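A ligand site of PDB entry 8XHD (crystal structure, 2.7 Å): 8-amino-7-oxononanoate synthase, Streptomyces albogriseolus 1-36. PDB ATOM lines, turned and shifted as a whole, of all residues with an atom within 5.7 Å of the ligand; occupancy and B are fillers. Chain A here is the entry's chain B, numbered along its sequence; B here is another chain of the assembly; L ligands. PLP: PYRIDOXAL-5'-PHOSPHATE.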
ATOM      1  N   TYR A  51     -15.208   9.947  28.365  1.00  0.00           N
ATOM      2  CA  TYR A  51     -14.080  10.330  29.199  1.00  0.00           C
ATOM      3  C   TYR A  51     -13.957  11.844  29.379  1.00  0.00           C
ATOM      4  O   TYR A  51     -13.193  12.285  30.244  1.00  0.00           O
ATOM      5  CB  TYR A  51     -12.769   9.789  28.619  1.00  0.00           C
ATOM      6  CG  TYR A  51     -12.621   8.275  28.674  1.00  0.00           C
ATOM      7  CD1 TYR A  51     -13.208   7.465  27.716  1.00  0.00           C
ATOM      8  CD2 TYR A  51     -11.882   7.671  29.681  1.00  0.00           C
ATOM      9  CE1 TYR A  51     -13.069   6.082  27.761  1.00  0.00           C
ATOM     10  CE2 TYR A  51     -11.735   6.294  29.736  1.00  0.00           C
ATOM     11  CZ  TYR A  51     -12.336   5.502  28.762  1.00  0.00           C
ATOM     12  OH  TYR A  51     -12.196   4.133  28.809  1.00  0.00           O
ATOM     13  N   ASN A 109       2.651  12.918  22.349  1.00  0.00           N
ATOM     14  CA  ASN A 109       1.444  12.600  21.588  1.00  0.00           C
ATOM     15  C   ASN A 109       0.486  11.684  22.346  1.00  0.00           C
ATOM     16  O   ASN A 109      -0.590  11.387  21.818  1.00  0.00           O
ATOM     17  CB  ASN A 109       1.829  11.968  20.243  1.00  0.00           C
ATOM     18  CG  ASN A 109       2.717  10.759  20.383  1.00  0.00           C
ATOM     19  OD1 ASN A 109       2.449   9.863  21.183  1.00  0.00           O
ATOM     20  ND2 ASN A 109       3.783  10.714  19.593  1.00  0.00           N
ATOM     21  N   SER A 110       0.851  11.236  23.551  1.00  0.00           N
ATOM     22  CA  SER A 110      -0.023  10.399  24.370  1.00  0.00           C
ATOM     23  C   SER A 110       0.584  10.274  25.760  1.00  0.00           C
ATOM     24  O   SER A 110       1.780  10.523  25.953  1.00  0.00           O
ATOM     25  CB  SER A 110      -0.214   8.999  23.754  1.00  0.00           C
ATOM     26  OG  SER A 110       0.977   8.244  23.813  1.00  0.00           O
ATOM     27  N   CYS A 111      -0.254   9.894  26.719  1.00  0.00           N
ATOM     28  CA  CYS A 111       0.241   9.556  28.048  1.00  0.00           C
ATOM     29  C   CYS A 111       1.047   8.264  28.005  1.00  0.00           C
ATOM     30  O   CYS A 111       1.997   8.100  28.781  1.00  0.00           O
ATOM     31  CB  CYS A 111      -0.917   9.440  29.028  1.00  0.00           C
ATOM     32  SG  CYS A 111      -0.437   9.075  30.728  1.00  0.00           S
ATOM     33  N   SER A 112       0.684   7.346  27.115  1.00  0.00           N
ATOM     34  CA  SER A 112       1.454   6.109  26.960  1.00  0.00           C
ATOM     35  C   SER A 112       2.875   6.409  26.507  1.00  0.00           C
ATOM     36  O   SER A 112       3.830   5.752  26.943  1.00  0.00           O
ATOM     37  CB  SER A 112       0.761   5.182  25.968  1.00  0.00           C
ATOM     38  OG  SER A 112      -0.575   4.929  26.365  1.00  0.00           O
ATOM     39  N   ALA A 113       3.039   7.402  25.623  1.00  0.00           N
ATOM     40  CA  ALA A 113       4.382   7.811  25.230  1.00  0.00           C
ATOM     41  C   ALA A 113       5.131   8.428  26.406  1.00  0.00           C
ATOM     42  O   ALA A 113       6.353   8.250  26.523  1.00  0.00           O
ATOM     43  CB  ALA A 113       4.308   8.803  24.070  1.00  0.00           C
ATOM     44  N   HIS A 142      -2.125   1.421  35.649  1.00  0.00           N
ATOM     45  CA  HIS A 142      -2.601   1.308  34.269  1.00  0.00           C
ATOM     46  C   HIS A 142      -1.572   0.590  33.397  1.00  0.00           C
ATOM     47  O   HIS A 142      -0.363   0.652  33.633  1.00  0.00           O
ATOM     48  CB  HIS A 142      -2.910   2.688  33.693  1.00  0.00           C
ATOM     49  CG  HIS A 142      -3.657   2.642  32.393  1.00  0.00           C
ATOM     50  ND1 HIS A 142      -3.022   2.543  31.173  1.00  0.00           N
ATOM     51  CD2 HIS A 142      -4.984   2.670  32.124  1.00  0.00           C
ATOM     52  CE1 HIS A 142      -3.931   2.518  30.216  1.00  0.00           C
ATOM     53  NE2 HIS A 142      -5.125   2.600  30.761  1.00  0.00           N
ATOM     54  N   CYS A 144      -0.467   1.016  30.453  1.00  0.00           N
ATOM     55  CA  CYS A 144       0.526   1.784  29.711  1.00  0.00           C
ATOM     56  C   CYS A 144       1.836   1.884  30.465  1.00  0.00           C
ATOM     57  O   CYS A 144       2.897   2.048  29.850  1.00  0.00           O
ATOM     58  CB  CYS A 144      -0.014   3.169  29.375  1.00  0.00           C
ATOM     59  SG  CYS A 144       0.075   4.354  30.730  1.00  0.00           S
ATOM     60  N   MET A 145       1.783   1.783  31.798  1.00  0.00           N
ATOM     61  CA  MET A 145       2.967   1.724  32.643  1.00  0.00           C
ATOM     62  C   MET A 145       3.405   0.293  32.944  1.00  0.00           C
ATOM     63  O   MET A 145       4.595  -0.003  32.952  1.00  0.00           O
ATOM     64  CB  MET A 145       2.707   2.461  33.959  1.00  0.00           C
ATOM     65  CG  MET A 145       2.420   3.946  33.814  1.00  0.00           C
ATOM     66  SD  MET A 145       1.800   4.684  35.344  1.00  0.00           S
ATOM     67  CE  MET A 145       0.276   3.773  35.574  1.00  0.00           C
ATOM     68  N   ASP A 184      -1.576   4.902  39.948  1.00  0.00           N
ATOM     69  CA  ASP A 184      -2.524   5.890  39.452  1.00  0.00           C
ATOM     70  C   ASP A 184      -3.011   6.750  40.602  1.00  0.00           C
ATOM     71  O   ASP A 184      -3.183   6.265  41.727  1.00  0.00           O
ATOM     72  CB  ASP A 184      -3.737   5.237  38.771  1.00  0.00           C
ATOM     73  CG  ASP A 184      -3.352   4.290  37.660  1.00  0.00           C
ATOM     74  OD1 ASP A 184      -2.176   3.882  37.611  1.00  0.00           O
ATOM     75  OD2 ASP A 184      -4.214   3.970  36.828  1.00  0.00           O
ATOM     76  N   VAL A 186      -6.049   8.165  40.501  1.00  0.00           N
ATOM     77  CA  VAL A 186      -7.435   7.721  40.576  1.00  0.00           C
ATOM     78  C   VAL A 186      -7.579   6.496  39.692  1.00  0.00           C
ATOM     79  O   VAL A 186      -7.177   6.516  38.529  1.00  0.00           O
ATOM     80  CB  VAL A 186      -8.404   8.830  40.140  1.00  0.00           C
ATOM     81  CG1 VAL A 186      -9.801   8.269  39.904  1.00  0.00           C
ATOM     82  CG2 VAL A 186      -8.451   9.933  41.183  1.00  0.00           C
ATOM     83  N   SER A 188      -9.877   3.808  37.717  1.00  0.00           N
ATOM     84  CA  SER A 188     -11.205   3.635  37.124  1.00  0.00           C
ATOM     85  C   SER A 188     -11.931   2.472  37.776  1.00  0.00           C
ATOM     86  O   SER A 188     -13.076   2.602  38.227  1.00  0.00           O
ATOM     87  CB  SER A 188     -11.075   3.429  35.620  1.00  0.00           C
ATOM     88  OG  SER A 188     -10.117   4.320  35.070  1.00  0.00           O
ATOM     89  N   ASP A 213       0.101   8.453  37.773  1.00  0.00           N
ATOM     90  CA  ASP A 213      -0.649   8.570  36.529  1.00  0.00           C
ATOM     91  C   ASP A 213      -1.939   9.315  36.856  1.00  0.00           C
ATOM     92  O   ASP A 213      -2.730   8.866  37.682  1.00  0.00           O
ATOM     93  CB  ASP A 213      -0.945   7.195  35.930  1.00  0.00           C
ATOM     94  CG  ASP A 213      -1.611   7.278  34.556  1.00  0.00           C
ATOM     95  OD1 ASP A 213      -2.303   8.271  34.256  1.00  0.00           O
ATOM     96  OD2 ASP A 213      -1.461   6.314  33.775  1.00  0.00           O
ATOM     97  N   ALA A 215      -4.366  10.475  34.549  1.00  0.00           N
ATOM     98  CA  ALA A 215      -5.257  10.557  33.395  1.00  0.00           C
ATOM     99  C   ALA A 215      -6.694  10.821  33.825  1.00  0.00           C
ATOM    100  O   ALA A 215      -7.427  11.559  33.152  1.00  0.00           O
ATOM    101  CB  ALA A 215      -5.160   9.282  32.567  1.00  0.00           C
ATOM    102  N   HIS A 216      -7.126  10.222  34.940  1.00  0.00           N
ATOM    103  CA  HIS A 216      -8.470  10.430  35.470  1.00  0.00           C
ATOM    104  C   HIS A 216      -8.477  11.363  36.677  1.00  0.00           C
ATOM    105  O   HIS A 216      -9.439  11.369  37.447  1.00  0.00           O
ATOM    106  CB  HIS A 216      -9.103   9.092  35.829  1.00  0.00           C
ATOM    107  CG  HIS A 216      -9.201   8.134  34.681  1.00  0.00           C
ATOM    108  ND1 HIS A 216     -10.176   8.228  33.713  1.00  0.00           N
ATOM    109  CD2 HIS A 216      -8.430   7.084  34.333  1.00  0.00           C
ATOM    110  CE1 HIS A 216     -10.009   7.274  32.821  1.00  0.00           C
ATOM    111  NE2 HIS A 216      -8.954   6.560  33.174  1.00  0.00           N
ATOM    112  N   THR A 244       0.167  12.193  32.509  1.00  0.00           N
ATOM    113  CA  THR A 244      -1.283  12.260  32.311  1.00  0.00           C
ATOM    114  C   THR A 244      -1.560  12.403  30.823  1.00  0.00           C
ATOM    115  O   THR A 244      -0.646  12.604  30.026  1.00  0.00           O
ATOM    116  CB  THR A 244      -1.904  13.420  33.097  1.00  0.00           C
ATOM    117  OG1 THR A 244      -3.328  13.427  32.909  1.00  0.00           O
ATOM    118  CG2 THR A 244      -1.339  14.756  32.639  1.00  0.00           C
ATOM    119  N   SER A 245      -2.828  12.255  30.465  1.00  0.00           N
ATOM    120  CA  SER A 245      -3.287  12.497  29.099  1.00  0.00           C
ATOM    121  C   SER A 245      -4.204  13.720  29.115  1.00  0.00           C
ATOM    122  O   SER A 245      -4.845  14.018  30.112  1.00  0.00           O
ATOM    123  CB  SER A 245      -4.021  11.278  28.528  1.00  0.00           C
ATOM    124  OG  SER A 245      -5.133  10.921  29.337  1.00  0.00           O
ATOM    125  N   LEU A 246      -4.242  14.426  27.980  1.00  0.00           N
ATOM    126  CA  LEU A 246      -4.962  15.695  27.905  1.00  0.00           C
ATOM    127  C   LEU A 246      -6.190  15.625  27.021  1.00  0.00           C
ATOM    128  O   LEU A 246      -6.760  16.667  26.694  1.00  0.00           O
ATOM    129  CB  LEU A 246      -4.012  16.799  27.419  1.00  0.00           C
ATOM    130  CG  LEU A 246      -2.709  16.916  28.197  1.00  0.00           C
ATOM    131  CD1 LEU A 246      -1.684  17.758  27.435  1.00  0.00           C
ATOM    132  CD2 LEU A 246      -2.931  17.496  29.589  1.00  0.00           C
ATOM    133  N   ASN A 247      -6.639  14.428  26.627  1.00  0.00           N
ATOM    134  CA  ASN A 247      -7.839  14.289  25.813  1.00  0.00           C
ATOM    135  C   ASN A 247      -9.065  13.923  26.634  1.00  0.00           C
ATOM    136  O   ASN A 247     -10.185  14.034  26.119  1.00  0.00           O
ATOM    137  CB  ASN A 247      -7.635  13.243  24.713  1.00  0.00           C
ATOM    138  CG  ASN A 247      -7.427  11.856  25.271  1.00  0.00           C
ATOM    139  OD1 ASN A 247      -6.890  11.680  26.371  1.00  0.00           O
ATOM    140  ND2 ASN A 247      -7.845  10.848  24.520  1.00  0.00           N
ATOM    141  N   LYS A 248      -8.883  13.480  27.866  1.00  0.00           N
ATOM    142  CA  LYS A 248      -9.983  13.174  28.764  1.00  0.00           C
ATOM    143  C   LYS A 248      -9.988  14.238  29.860  1.00  0.00           C
ATOM    144  O   LYS A 248      -8.974  14.453  30.530  1.00  0.00           O
ATOM    145  CB  LYS A 248      -9.831  11.772  29.352  1.00  0.00           C
ATOM    146  CG  LYS A 248      -8.487  11.497  30.006  1.00  0.00           C
ATOM    147  CD  LYS A 248      -8.325  10.034  30.382  1.00  0.00           C
ATOM    148  CE  LYS A 248      -8.202   9.171  29.141  1.00  0.00           C
ATOM    149  NZ  LYS A 248      -8.089   7.736  29.492  1.00  0.00           N
ATOM    150  N   GLY A 254      -3.349  14.382  23.268  1.00  0.00           N
ATOM    151  CA  GLY A 254      -2.004  14.032  23.668  1.00  0.00           C
ATOM    152  C   GLY A 254      -1.865  13.816  25.169  1.00  0.00           C
ATOM    153  O   GLY A 254      -2.842  13.676  25.917  1.00  0.00           O
ATOM    154  N   GLY A 255      -0.610  13.788  25.602  1.00  0.00           N
ATOM    155  CA  GLY A 255      -0.290  13.579  26.997  1.00  0.00           C
ATOM    156  C   GLY A 255       0.768  14.548  27.489  1.00  0.00           C
ATOM    157  O   GLY A 255       1.148  15.476  26.771  1.00  0.00           O
ATOM    158  N   ASN B 109      -1.302   6.970  17.045  1.00  0.00           N
ATOM    159  CA  ASN B 109      -0.737   8.274  17.361  1.00  0.00           C
ATOM    160  C   ASN B 109       0.635   8.454  16.719  1.00  0.00           C
ATOM    161  O   ASN B 109       1.025   9.580  16.385  1.00  0.00           O
ATOM    162  CB  ASN B 109      -0.620   8.472  18.876  1.00  0.00           C
ATOM    163  CG  ASN B 109      -1.891   8.120  19.620  1.00  0.00           C
ATOM    164  OD1 ASN B 109      -1.867   7.289  20.544  1.00  0.00           O
ATOM    165  ND2 ASN B 109      -3.008   8.740  19.245  1.00  0.00           N
ATOM    166  N   TRP B 280      -5.459   0.799  24.398  1.00  0.00           N
ATOM    167  CA  TRP B 280      -5.547   1.729  25.517  1.00  0.00           C
ATOM    168  C   TRP B 280      -5.092   3.155  25.207  1.00  0.00           C
ATOM    169  O   TRP B 280      -5.264   4.029  26.067  1.00  0.00           O
ATOM    170  CB  TRP B 280      -4.747   1.199  26.726  1.00  0.00           C
ATOM    171  CG  TRP B 280      -3.230   1.204  26.568  1.00  0.00           C
ATOM    172  CD1 TRP B 280      -2.434   2.256  26.200  1.00  0.00           C
ATOM    173  CD2 TRP B 280      -2.345   0.120  26.829  1.00  0.00           C
ATOM    174  NE1 TRP B 280      -1.121   1.884  26.193  1.00  0.00           N
ATOM    175  CE2 TRP B 280      -1.028   0.574  26.575  1.00  0.00           C
ATOM    176  CE3 TRP B 280      -2.528  -1.202  27.247  1.00  0.00           C
ATOM    177  CZ2 TRP B 280       0.085  -0.242  26.728  1.00  0.00           C
ATOM    178  CZ3 TRP B 280      -1.421  -2.009  27.392  1.00  0.00           C
ATOM    179  CH2 TRP B 280      -0.125  -1.532  27.132  1.00  0.00           C
ATOM    180  N   SER B 281      -4.501   3.416  24.045  1.00  0.00           N
ATOM    181  CA  SER B 281      -3.980   4.738  23.737  1.00  0.00           C
ATOM    182  C   SER B 281      -4.902   5.480  22.777  1.00  0.00           C
ATOM    183  O   SER B 281      -5.587   4.870  21.955  1.00  0.00           O
ATOM    184  CB  SER B 281      -2.561   4.665  23.146  1.00  0.00           C
ATOM    185  OG  SER B 281      -1.962   5.939  23.122  1.00  0.00           O
ATOM    186  N   GLN B 282      -4.897   6.802  22.891  1.00  0.00           N
ATOM    187  CA  GLN B 282      -5.861   7.638  22.180  1.00  0.00           C
ATOM    188  C   GLN B 282      -5.684   7.516  20.667  1.00  0.00           C
ATOM    189  O   GLN B 282      -4.632   7.120  20.158  1.00  0.00           O
ATOM    190  CB  GLN B 282      -5.709   9.089  22.612  1.00  0.00           C
ATOM    191  CG  GLN B 282      -4.281   9.613  22.609  1.00  0.00           C
ATOM    192  CD  GLN B 282      -4.184  11.022  23.148  1.00  0.00           C
ATOM    193  OE1 GLN B 282      -4.615  11.975  22.509  1.00  0.00           O
ATOM    194  NE2 GLN B 282      -3.614  11.158  24.346  1.00  0.00           N
HETATM  195  N1  PLP L   1      -3.418   6.059  32.216  1.00  0.00           N
HETATM  196  C2  PLP L   1      -4.773   5.884  32.393  1.00  0.00           C
HETATM  197  C2A PLP L   1      -5.316   5.723  33.782  1.00  0.00           C
HETATM  198  C3  PLP L   1      -5.631   5.876  31.305  1.00  0.00           C
HETATM  199  O3  PLP L   1      -6.971   5.699  31.491  1.00  0.00           O
HETATM  200  C4  PLP L   1      -5.128   6.026  30.006  1.00  0.00           C
HETATM  201  C4A PLP L   1      -5.976   5.514  28.880  1.00  0.00           C
HETATM  202  O4A PLP L   1      -6.840   4.652  29.067  1.00  0.00           O
HETATM  203  C5  PLP L   1      -3.759   6.200  29.829  1.00  0.00           C
HETATM  204  C6  PLP L   1      -2.915   6.206  30.938  1.00  0.00           C
HETATM  205  C5A PLP L   1      -3.137   6.375  28.460  1.00  0.00           C
HETATM  206  O4P PLP L   1      -3.928   7.212  27.632  1.00  0.00           O
HETATM  207  P   PLP L   1      -3.320   7.824  26.271  1.00  0.00           P
HETATM  208  O1P PLP L   1      -2.881   9.250  26.488  1.00  0.00           O
HETATM  209  O2P PLP L   1      -4.378   7.770  25.181  1.00  0.00           O
HETATM  210  O3P PLP L   1      -2.146   6.966  25.838  1.00  0.00           O
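N of Ala 215 lies within hydrogen-bond range of OD1 of Asp 213, at 3.0 Å.
The side-chain amide oxygen (OE1) of Gln 282 of chain B sits at hydrogen-bond distance from the backbone NH (N) of Gly 254, 2.8 Å away.
NE1 of Trp 280 of chain B sits at hydrogen-bond distance from OG of Ser 112 (3.1 Å).
OG of Ser 281 of chain B is in hydrogen-bond range of OD1 of Asn 109 of chain B, at 2.9 Å.
N of Cys 144 is in hydrogen-bond range of ND1 of His 142, 3.1 Å away.
OD1 of Asp 184 sits at hydrogen-bond distance from N of His 142 (3.1 Å).
OG of Ser 110 is in hydrogen-bond range of N of Ala 113.
OG of Ser 110 lies within hydrogen-bond range of OD1 of Asn 109 of chain A (3.4 Å).
N1 of the ligand sits at hydrogen-bond distance from OD2 of Asp 213 (2.5 Å).
The backbone NH (N) of Gln 282 of chain B is in hydrogen-bond range of an oxygen (O2P) of the ligand, 2.5 Å away.
O1P of the ligand lies within hydrogen-bond range of NE2 of Gln 282 of chain B, 3.0 Å away.
The backbone NH (N) of Ser 112 is in hydrogen-bond range of an oxygen (O3P) of the ligand.
O3P of the ligand lies within hydrogen-bond range of OG of Ser 112 (2.6 Å).
N of Cys 111 sits at hydrogen-bond distance from O1P of the ligand (2.7 Å).
NE2 of His 216 is in hydrogen-bond range of O3 of the ligand (2.7 Å).
OG of Ser 281 of chain B lies within hydrogen-bond range of O3P of the ligand.
The side-chain amino group (NZ) of Lys 248 sits at hydrogen-bond distance from an oxygen (O3) of the ligand.
NE2 of His 142 lies within hydrogen-bond range of O4A of the ligand (3.2 Å).
The backbone carbonyl oxygen of Trp 280 of chain B lies close to an oxygen (O4A) of the ligand, 3.4 Å away.
Merely in contact with the ligand: Ser 110, Cys 144, Asp 184, Ala 215 and Ser 245.
Along chain A the residues within 4 Å of the ligand span positions 110 to 248.
The nearest printed residue that does not touch the ligand is Gly 254 (4.5 Å).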
